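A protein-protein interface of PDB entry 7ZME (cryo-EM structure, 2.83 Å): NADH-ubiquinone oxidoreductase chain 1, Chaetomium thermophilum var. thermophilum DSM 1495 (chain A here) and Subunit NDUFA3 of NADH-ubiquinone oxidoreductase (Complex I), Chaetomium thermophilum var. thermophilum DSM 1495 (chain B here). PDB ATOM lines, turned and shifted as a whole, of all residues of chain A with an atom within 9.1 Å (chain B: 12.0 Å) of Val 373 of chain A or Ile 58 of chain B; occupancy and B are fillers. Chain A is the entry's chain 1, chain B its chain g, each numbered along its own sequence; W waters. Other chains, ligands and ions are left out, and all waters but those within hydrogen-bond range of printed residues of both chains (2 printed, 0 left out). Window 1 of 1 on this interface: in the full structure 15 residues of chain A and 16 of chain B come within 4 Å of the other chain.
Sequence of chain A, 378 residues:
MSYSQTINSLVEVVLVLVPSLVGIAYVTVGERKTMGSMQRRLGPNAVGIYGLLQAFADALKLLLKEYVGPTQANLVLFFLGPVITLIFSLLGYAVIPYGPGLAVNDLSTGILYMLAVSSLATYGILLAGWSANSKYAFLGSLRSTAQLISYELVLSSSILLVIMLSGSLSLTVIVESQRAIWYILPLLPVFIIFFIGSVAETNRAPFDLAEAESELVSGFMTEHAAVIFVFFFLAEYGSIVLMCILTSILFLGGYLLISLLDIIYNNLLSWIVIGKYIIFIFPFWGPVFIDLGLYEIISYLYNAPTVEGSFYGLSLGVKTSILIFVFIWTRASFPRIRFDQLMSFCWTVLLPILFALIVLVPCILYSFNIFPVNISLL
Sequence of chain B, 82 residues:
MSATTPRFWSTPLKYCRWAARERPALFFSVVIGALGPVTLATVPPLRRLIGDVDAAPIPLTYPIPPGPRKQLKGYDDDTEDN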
ATOM      1  N   ILE A 163      30.609  -9.421 -11.058  1.00  0.00           N
ATOM      2  CA  ILE A 163      29.484 -10.131 -11.659  1.00  0.00           C
ATOM      3  C   ILE A 163      29.938 -11.443 -12.281  1.00  0.00           C
ATOM      4  O   ILE A 163      29.161 -12.400 -12.367  1.00  0.00           O
ATOM      5  CB  ILE A 163      28.774  -9.238 -12.695  1.00  0.00           C
ATOM      6  CG1 ILE A 163      28.635  -7.805 -12.175  1.00  0.00           C
ATOM      7  CG2 ILE A 163      27.420  -9.821 -13.070  1.00  0.00           C
ATOM      8  CD1 ILE A 163      27.827  -7.674 -10.910  1.00  0.00           C
ATOM      9  N   MET A 164      31.171 -11.498 -12.773  1.00  0.00           N
ATOM     10  CA  MET A 164      31.690 -12.732 -13.406  1.00  0.00           C
ATOM     11  C   MET A 164      31.798 -13.835 -12.351  1.00  0.00           C
ATOM     12  O   MET A 164      31.845 -15.000 -12.735  1.00  0.00           O
ATOM     13  CB  MET A 164      33.048 -12.483 -14.053  1.00  0.00           C
ATOM     14  CG  MET A 164      32.978 -11.749 -15.372  1.00  0.00           C
ATOM     15  SD  MET A 164      34.625 -11.317 -15.986  1.00  0.00           S
ATOM     16  CE  MET A 164      34.210 -10.627 -17.585  1.00  0.00           C
ATOM     17  N   LEU A 165      31.834 -13.475 -11.067  1.00  0.00           N
ATOM     18  CA  LEU A 165      31.871 -14.489  -9.981  1.00  0.00           C
ATOM     19  C   LEU A 165      30.465 -14.754  -9.442  1.00  0.00           C
ATOM     20  O   LEU A 165      30.168 -15.916  -9.213  1.00  0.00           O
ATOM     21  CB  LEU A 165      32.770 -14.004  -8.841  1.00  0.00           C
ATOM     22  CG  LEU A 165      34.233 -13.719  -9.161  1.00  0.00           C
ATOM     23  CD1 LEU A 165      35.017 -13.593  -7.866  1.00  0.00           C
ATOM     24  CD2 LEU A 165      34.824 -14.820 -10.019  1.00  0.00           C
ATOM     25  N   SER A 166      29.651 -13.721  -9.228  1.00  0.00           N
ATOM     26  CA  SER A 166      28.295 -13.885  -8.633  1.00  0.00           C
ATOM     27  C   SER A 166      27.310 -14.382  -9.690  1.00  0.00           C
ATOM     28  O   SER A 166      26.446 -15.190  -9.335  1.00  0.00           O
ATOM     29  CB  SER A 166      27.839 -12.595  -8.021  1.00  0.00           C
ATOM     30  OG  SER A 166      27.783 -11.565  -8.993  1.00  0.00           O
ATOM     31  N   GLY A 167      27.436 -13.896 -10.930  1.00  0.00           N
ATOM     32  CA  GLY A 167      26.551 -14.279 -12.044  1.00  0.00           C
ATOM     33  C   GLY A 167      25.176 -13.670 -11.923  1.00  0.00           C
ATOM     34  O   GLY A 167      24.272 -14.158 -12.616  1.00  0.00           O
ATOM     35  N   SER A 168      25.012 -12.626 -11.101  1.00  0.00           N
ATOM     36  CA  SER A 168      23.631 -12.150 -10.842  1.00  0.00           C
ATOM     37  C   SER A 168      23.286 -10.723 -11.265  1.00  0.00           C
ATOM     38  O   SER A 168      22.285 -10.623 -12.003  1.00  0.00           O
ATOM     39  CB  SER A 168      23.264 -12.364  -9.417  1.00  0.00           C
ATOM     40  OG  SER A 168      21.875 -12.151  -9.241  1.00  0.00           O
ATOM     41  N   VAL A 173      22.053 -11.343  -4.121  1.00  0.00           N
ATOM     42  CA  VAL A 173      22.706 -12.595  -4.591  1.00  0.00           C
ATOM     43  C   VAL A 173      24.227 -12.479  -4.471  1.00  0.00           C
ATOM     44  O   VAL A 173      24.873 -13.496  -4.222  1.00  0.00           O
ATOM     45  CB  VAL A 173      22.229 -12.999  -5.996  1.00  0.00           C
ATOM     46  CG1 VAL A 173      22.803 -14.342  -6.417  1.00  0.00           C
ATOM     47  CG2 VAL A 173      20.714 -13.037  -6.072  1.00  0.00           C
ATOM     48  N   SER A 177      26.429 -14.953  -2.334  1.00  0.00           N
ATOM     49  CA  SER A 177      27.566 -15.675  -2.957  1.00  0.00           C
ATOM     50  C   SER A 177      28.801 -15.605  -2.052  1.00  0.00           C
ATOM     51  O   SER A 177      29.572 -16.566  -2.047  1.00  0.00           O
ATOM     52  CB  SER A 177      27.828 -15.141  -4.333  1.00  0.00           C
ATOM     53  OG  SER A 177      26.694 -15.310  -5.165  1.00  0.00           O
ATOM     54  N   ASN A 369      36.262 -25.200 -13.650  1.00  0.00           N
ATOM     55  CA  ASN A 369      34.813 -25.546 -13.683  1.00  0.00           C
ATOM     56  C   ASN A 369      34.046 -24.689 -12.684  1.00  0.00           C
ATOM     57  O   ASN A 369      33.132 -25.215 -12.043  1.00  0.00           O
ATOM     58  CB  ASN A 369      34.532 -27.036 -13.472  1.00  0.00           C
ATOM     59  CG  ASN A 369      33.218 -27.482 -14.071  1.00  0.00           C
ATOM     60  OD1 ASN A 369      32.561 -28.369 -13.537  1.00  0.00           O
ATOM     61  ND2 ASN A 369      32.821 -26.862 -15.169  1.00  0.00           N
ATOM     62  N   ILE A 370      34.434 -23.420 -12.547  1.00  0.00           N
ATOM     63  CA  ILE A 370      33.797 -22.562 -11.509  1.00  0.00           C
ATOM     64  C   ILE A 370      32.934 -21.450 -12.095  1.00  0.00           C
ATOM     65  O   ILE A 370      32.872 -20.391 -11.468  1.00  0.00           O
ATOM     66  CB  ILE A 370      34.758 -22.128 -10.378  1.00  0.00           C
ATOM     67  CG1 ILE A 370      36.070 -21.535 -10.892  1.00  0.00           C
ATOM     68  CG2 ILE A 370      35.002 -23.290  -9.429  1.00  0.00           C
ATOM     69  CD1 ILE A 370      36.828 -20.769  -9.841  1.00  0.00           C
ATOM     70  N   PHE A 371      32.313 -21.653 -13.256  1.00  0.00           N
ATOM     71  CA  PHE A 371      31.350 -20.636 -13.765  1.00  0.00           C
ATOM     72  C   PHE A 371      30.071 -20.763 -12.932  1.00  0.00           C
ATOM     73  O   PHE A 371      29.514 -21.861 -12.833  1.00  0.00           O
ATOM     74  CB  PHE A 371      31.029 -20.798 -15.255  1.00  0.00           C
ATOM     75  CG  PHE A 371      32.012 -20.196 -16.225  1.00  0.00           C
ATOM     76  CD1 PHE A 371      32.695 -19.030 -15.923  1.00  0.00           C
ATOM     77  CD2 PHE A 371      32.224 -20.776 -17.464  1.00  0.00           C
ATOM     78  CE1 PHE A 371      33.580 -18.471 -16.830  1.00  0.00           C
ATOM     79  CE2 PHE A 371      33.110 -20.217 -18.370  1.00  0.00           C
ATOM     80  CZ  PHE A 371      33.788 -19.066 -18.051  1.00  0.00           C
ATOM     81  N   PRO A 372      29.595 -19.672 -12.303  1.00  0.00           N
ATOM     82  CA  PRO A 372      28.364 -19.713 -11.522  1.00  0.00           C
ATOM     83  C   PRO A 372      27.093 -19.952 -12.355  1.00  0.00           C
ATOM     84  O   PRO A 372      27.008 -19.459 -13.454  1.00  0.00           O
ATOM     85  CB  PRO A 372      28.352 -18.326 -10.862  1.00  0.00           C
ATOM     86  CG  PRO A 372      29.111 -17.452 -11.824  1.00  0.00           C
ATOM     87  CD  PRO A 372      30.221 -18.348 -12.321  1.00  0.00           C
ATOM     88  N   VAL A 373      26.162 -20.735 -11.816  1.00  0.00           N
ATOM     89  CA  VAL A 373      24.847 -20.932 -12.490  1.00  0.00           C
ATOM     90  C   VAL A 373      24.156 -19.570 -12.511  1.00  0.00           C
ATOM     91  O   VAL A 373      24.236 -18.857 -11.502  1.00  0.00           O
ATOM     92  CB  VAL A 373      23.996 -22.055 -11.865  1.00  0.00           C
ATOM     93  CG1 VAL A 373      24.498 -23.432 -12.254  1.00  0.00           C
ATOM     94  CG2 VAL A 373      23.906 -21.928 -10.354  1.00  0.00           C
ATOM     95  N   ASN A 374      23.515 -19.212 -13.616  1.00  0.00           N
ATOM     96  CA  ASN A 374      22.968 -17.840 -13.768  1.00  0.00           C
ATOM     97  C   ASN A 374      21.466 -17.896 -13.523  1.00  0.00           C
ATOM     98  O   ASN A 374      20.759 -16.973 -13.933  1.00  0.00           O
ATOM     99  CB  ASN A 374      23.509 -17.187 -15.037  1.00  0.00           C
ATOM    100  CG  ASN A 374      25.021 -17.154 -15.060  1.00  0.00           C
ATOM    101  OD1 ASN A 374      25.640 -16.279 -14.470  1.00  0.00           O
ATOM    102  ND2 ASN A 374      25.625 -18.115 -15.730  1.00  0.00           N
ATOM    103  N   ILE A 375      21.031 -18.946 -12.841  1.00  0.00           N
ATOM    104  CA  ILE A 375      19.596 -19.146 -12.522  1.00  0.00           C
ATOM    105  C   ILE A 375      19.340 -18.472 -11.180  1.00  0.00           C
ATOM    106  O   ILE A 375      20.316 -18.030 -10.558  1.00  0.00           O
ATOM    107  CB  ILE A 375      19.335 -20.664 -12.424  1.00  0.00           C
ATOM    108  CG1 ILE A 375      20.001 -21.290 -11.199  1.00  0.00           C
ATOM    109  CG2 ILE A 375      19.739 -21.372 -13.706  1.00  0.00           C
ATOM    110  CD1 ILE A 375      19.521 -22.686 -10.898  1.00  0.00           C
ATOM    111  N   SER A 376      18.079 -18.361 -10.775  1.00  0.00           N
ATOM    112  CA  SER A 376      17.794 -17.835  -9.416  1.00  0.00           C
ATOM    113  C   SER A 376      18.009 -18.972  -8.419  1.00  0.00           C
ATOM    114  O   SER A 376      17.398 -20.032  -8.599  1.00  0.00           O
ATOM    115  CB  SER A 376      16.409 -17.278  -9.308  1.00  0.00           C
ATOM    116  OG  SER A 376      16.231 -16.182 -10.188  1.00  0.00           O
ATOM    117  N   LEU A 377      18.849 -18.758  -7.413  1.00  0.00           N
ATOM    118  CA  LEU A 377      19.138 -19.786  -6.384  1.00  0.00           C
ATOM    119  C   LEU A 377      19.332 -19.071  -5.054  1.00  0.00           C
ATOM    120  O   LEU A 377      18.515 -19.273  -4.144  1.00  0.00           O
ATOM    121  CB  LEU A 377      20.407 -20.543  -6.783  1.00  0.00           C
ATOM    122  CG  LEU A 377      20.885 -21.622  -5.816  1.00  0.00           C
ATOM    123  CD1 LEU A 377      19.992 -22.849  -5.888  1.00  0.00           C
ATOM    124  CD2 LEU A 377      22.327 -21.997  -6.111  1.00  0.00           C
ATOM    125  N   LEU A 378      20.407 -18.295  -4.946  1.00  0.00           N
ATOM    126  CA  LEU A 378      20.722 -17.602  -3.673  1.00  0.00           C
ATOM    127  C   LEU A 378      19.946 -16.278  -3.608  1.00  0.00           C
ATOM    128  O   LEU A 378      19.365 -16.011  -2.545  1.00  0.00           O
ATOM    129  CB  LEU A 378      22.238 -17.381  -3.603  1.00  0.00           C
ATOM    130  CG  LEU A 378      23.105 -18.636  -3.688  1.00  0.00           C
ATOM    131  CD1 LEU A 378      24.578 -18.281  -3.609  1.00  0.00           C
ATOM    132  CD2 LEU A 378      22.751 -19.619  -2.587  1.00  0.00           C
ATOM    133  N   VAL B  53      37.147 -33.781 -12.126  1.00  0.00           N
ATOM    134  CA  VAL B  53      36.223 -34.040 -13.257  1.00  0.00           C
ATOM    135  C   VAL B  53      35.296 -32.842 -13.409  1.00  0.00           C
ATOM    136  O   VAL B  53      34.689 -32.444 -12.406  1.00  0.00           O
ATOM    137  CB  VAL B  53      35.432 -35.342 -13.025  1.00  0.00           C
ATOM    138  CG1 VAL B  53      34.411 -35.595 -14.123  1.00  0.00           C
ATOM    139  CG2 VAL B  53      36.351 -36.544 -12.878  1.00  0.00           C
ATOM    140  N   ASP B  54      35.181 -32.302 -14.619  1.00  0.00           N
ATOM    141  CA  ASP B  54      34.198 -31.221 -14.869  1.00  0.00           C
ATOM    142  C   ASP B  54      32.840 -31.851 -14.564  1.00  0.00           C
ATOM    143  O   ASP B  54      32.622 -33.001 -14.980  1.00  0.00           O
ATOM    144  CB  ASP B  54      34.330 -30.762 -16.322  1.00  0.00           C
ATOM    145  CG  ASP B  54      33.403 -29.655 -16.797  1.00  0.00           C
ATOM    146  OD1 ASP B  54      32.286 -29.544 -16.272  1.00  0.00           O
ATOM    147  OD2 ASP B  54      33.809 -28.913 -17.713  1.00  0.00           O
ATOM    148  N   ALA B  55      31.966 -31.129 -13.864  1.00  0.00           N
ATOM    149  CA  ALA B  55      30.664 -31.703 -13.473  1.00  0.00           C
ATOM    150  C   ALA B  55      29.742 -31.765 -14.682  1.00  0.00           C
ATOM    151  O   ALA B  55      30.043 -31.110 -15.693  1.00  0.00           O
ATOM    152  CB  ALA B  55      30.059 -30.888 -12.365  1.00  0.00           C
ATOM    153  N   ALA B  56      28.671 -32.547 -14.583  1.00  0.00           N
ATOM    154  CA  ALA B  56      27.656 -32.598 -15.655  1.00  0.00           C
ATOM    155  C   ALA B  56      26.805 -31.330 -15.596  1.00  0.00           C
ATOM    156  O   ALA B  56      26.573 -30.828 -14.491  1.00  0.00           O
ATOM    157  CB  ALA B  56      26.811 -33.817 -15.453  1.00  0.00           C
ATOM    158  N   PRO B  57      26.342 -30.776 -16.731  1.00  0.00           N
ATOM    159  CA  PRO B  57      25.454 -29.620 -16.698  1.00  0.00           C
ATOM    160  C   PRO B  57      24.147 -29.823 -15.904  1.00  0.00           C
ATOM    161  O   PRO B  57      23.556 -30.872 -16.019  1.00  0.00           O
ATOM    162  CB  PRO B  57      25.179 -29.361 -18.184  1.00  0.00           C
ATOM    163  CG  PRO B  57      25.489 -30.671 -18.866  1.00  0.00           C
ATOM    164  CD  PRO B  57      26.658 -31.223 -18.085  1.00  0.00           C
ATOM    165  N   ILE B  58      23.720 -28.810 -15.140  1.00  0.00           N
ATOM    166  CA  ILE B  58      22.424 -28.891 -14.403  1.00  0.00           C
ATOM    167  C   ILE B  58      21.257 -28.785 -15.401  1.00  0.00           C
ATOM    168  O   ILE B  58      21.420 -28.058 -16.391  1.00  0.00           O
ATOM    169  CB  ILE B  58      22.320 -27.854 -13.264  1.00  0.00           C
ATOM    170  CG1 ILE B  58      22.099 -26.431 -13.782  1.00  0.00           C
ATOM    171  CG2 ILE B  58      23.523 -27.945 -12.340  1.00  0.00           C
ATOM    172  CD1 ILE B  58      21.455 -25.516 -12.777  1.00  0.00           C
ATOM    173  N   PRO B  59      20.107 -29.490 -15.247  1.00  0.00           N
ATOM    174  CA  PRO B  59      19.047 -29.418 -16.262  1.00  0.00           C
ATOM    175  C   PRO B  59      18.341 -28.071 -16.233  1.00  0.00           C
ATOM    176  O   PRO B  59      17.851 -27.630 -15.192  1.00  0.00           O
ATOM    177  CB  PRO B  59      18.104 -30.561 -15.871  1.00  0.00           C
ATOM    178  CG  PRO B  59      18.364 -30.794 -14.433  1.00  0.00           C
ATOM    179  CD  PRO B  59      19.801 -30.470 -14.194  1.00  0.00           C
ATOM    180  N   LEU B  60      18.219 -27.442 -17.394  1.00  0.00           N
ATOM    181  CA  LEU B  60      17.546 -26.120 -17.503  1.00  0.00           C
ATOM    182  C   LEU B  60      16.316 -26.279 -18.397  1.00  0.00           C
ATOM    183  O   LEU B  60      15.801 -25.262 -18.847  1.00  0.00           O
ATOM    184  CB  LEU B  60      18.550 -25.090 -18.030  1.00  0.00           C
ATOM    185  CG  LEU B  60      19.812 -24.915 -17.189  1.00  0.00           C
ATOM    186  CD1 LEU B  60      20.766 -23.935 -17.843  1.00  0.00           C
ATOM    187  CD2 LEU B  60      19.453 -24.453 -15.793  1.00  0.00           C
ATOM    188  N   THR B  61      15.835 -27.508 -18.575  1.00  0.00           N
ATOM    189  CA  THR B  61      14.585 -27.839 -19.312  1.00  0.00           C
ATOM    190  C   THR B  61      14.202 -29.225 -18.792  1.00  0.00           C
ATOM    191  O   THR B  61      15.084 -29.885 -18.241  1.00  0.00           O
ATOM    192  CB  THR B  61      14.748 -27.836 -20.842  1.00  0.00           C
ATOM    193  OG1 THR B  61      13.460 -27.922 -21.449  1.00  0.00           O
ATOM    194  CG2 THR B  61      15.628 -28.947 -21.366  1.00  0.00           C
ATOM    195  N   TYR B  62      12.919 -29.579 -18.820  1.00  0.00           N
ATOM    196  CA  TYR B  62      12.504 -30.931 -18.378  1.00  0.00           C
ATOM    197  C   TYR B  62      13.275 -31.966 -19.192  1.00  0.00           C
ATOM    198  O   TYR B  62      13.275 -31.902 -20.428  1.00  0.00           O
ATOM    199  CB  TYR B  62      10.997 -31.135 -18.535  1.00  0.00           C
ATOM    200  CG  TYR B  62      10.461 -32.367 -17.854  1.00  0.00           C
ATOM    201  CD1 TYR B  62      10.530 -33.612 -18.458  1.00  0.00           C
ATOM    202  CD2 TYR B  62       9.890 -32.289 -16.596  1.00  0.00           C
ATOM    203  CE1 TYR B  62      10.056 -34.748 -17.828  1.00  0.00           C
ATOM    204  CE2 TYR B  62       9.402 -33.414 -15.957  1.00  0.00           C
ATOM    205  CZ  TYR B  62       9.485 -34.648 -16.574  1.00  0.00           C
ATOM    206  OH  TYR B  62       9.001 -35.756 -15.946  1.00  0.00           O
ATOM    207  N   PRO B  63      13.917 -32.948 -18.531  1.00  0.00           N
ATOM    208  CA  PRO B  63      14.709 -33.950 -19.228  1.00  0.00           C
ATOM    209  C   PRO B  63      13.767 -34.987 -19.844  1.00  0.00           C
ATOM    210  O   PRO B  63      13.368 -35.885 -19.144  1.00  0.00           O
ATOM    211  CB  PRO B  63      15.553 -34.567 -18.107  1.00  0.00           C
ATOM    212  CG  PRO B  63      15.351 -33.661 -16.914  1.00  0.00           C
ATOM    213  CD  PRO B  63      13.952 -33.120 -17.084  1.00  0.00           C
ATOM    214  N   ILE B  64      13.438 -34.831 -21.126  1.00  0.00           N
ATOM    215  CA  ILE B  64      12.445 -35.739 -21.757  1.00  0.00           C
ATOM    216  C   ILE B  64      13.152 -37.056 -22.076  1.00  0.00           C
ATOM    217  O   ILE B  64      14.133 -37.000 -22.832  1.00  0.00           O
ATOM    218  CB  ILE B  64      11.770 -35.111 -22.990  1.00  0.00           C
ATOM    219  CG1 ILE B  64      11.108 -33.769 -22.667  1.00  0.00           C
ATOM    220  CG2 ILE B  64      10.778 -36.087 -23.604  1.00  0.00           C
ATOM    221  CD1 ILE B  64       9.714 -33.896 -22.113  1.00  0.00           C
HETATM  222  O   HOH W   1      29.875 -27.890 -15.676  1.00  0.00           O
HETATM  223  O   HOH W   2      35.744 -26.612 -16.936  1.00  0.00           O
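Of the 12 printed residues of chain B, 4 touch a printed residue of chain A. Printed residues of chain A that touch a printed residue of chain B: Asn 369, Val 373 and Ile 375. Hydrophobic or aromatic side chains of chain A within 4 Å of the printed part of chain B: Val 373 and Ile 375.
Met 164 of chain A touches none of the printed residues of chain B. No residue of chain B comes within 4 Å of Gly 167 of chain A. Printed residues of chain B within 4 Å of Asn 369 of chain A: Asp 54 and Ala 55. Val 373 of chain A touches one residue of chain B. No residue of chain B comes within 4 Å of Asn 374 of chain A. Ile 375 of chain A touches two residues of chain B. Val 53 of chain B touches none of the printed residues of chain A. Printed residues of chain A within 4 Å of Asp 54 of chain B: Asn 369 (2.9 Å). Pro 57 of chain B touches none of the printed residues of chain A. Ile 58 of chain B touches two residues of chain A. Pro 59 of chain B touches none of the printed residues of chain A. Of the printed residues of chain A, Leu 60 of chain B touches Ile 375 (3.7 Å).
OD1 of Asn 369 of chain A sits at hydrogen-bond distance from N of Ala 55 of chain B (2.8 Å). The side-chain carboxylate (OD1) of Asp 54 of chain B lies within hydrogen-bond range of the side-chain amide nitrogen (ND2) of Asn 369 of chain A (2.9 Å).
Among the printed residues, merely in contact across the chains: Val 373 of chain A with Ile 58 of chain B (3.7 Å), Ile 375 of chain A with Ile 58 of chain B (3.9 Å) and Ile 375 of chain A with Leu 60 of chain B (3.7 Å).
Water W1 lies within hydrogen-bond range of OD1 of Asp 54 of chain B (3.0 Å), ND2 of Asn 369 of chain A (3.2 Å) and O of Ala 55 of chain B (3.2 Å). Water W2 lies within hydrogen-bond range of OD2 of Asp 54 of chain B (3.1 Å) and ND2 of Asn 369 of chain A (3.4 Å).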
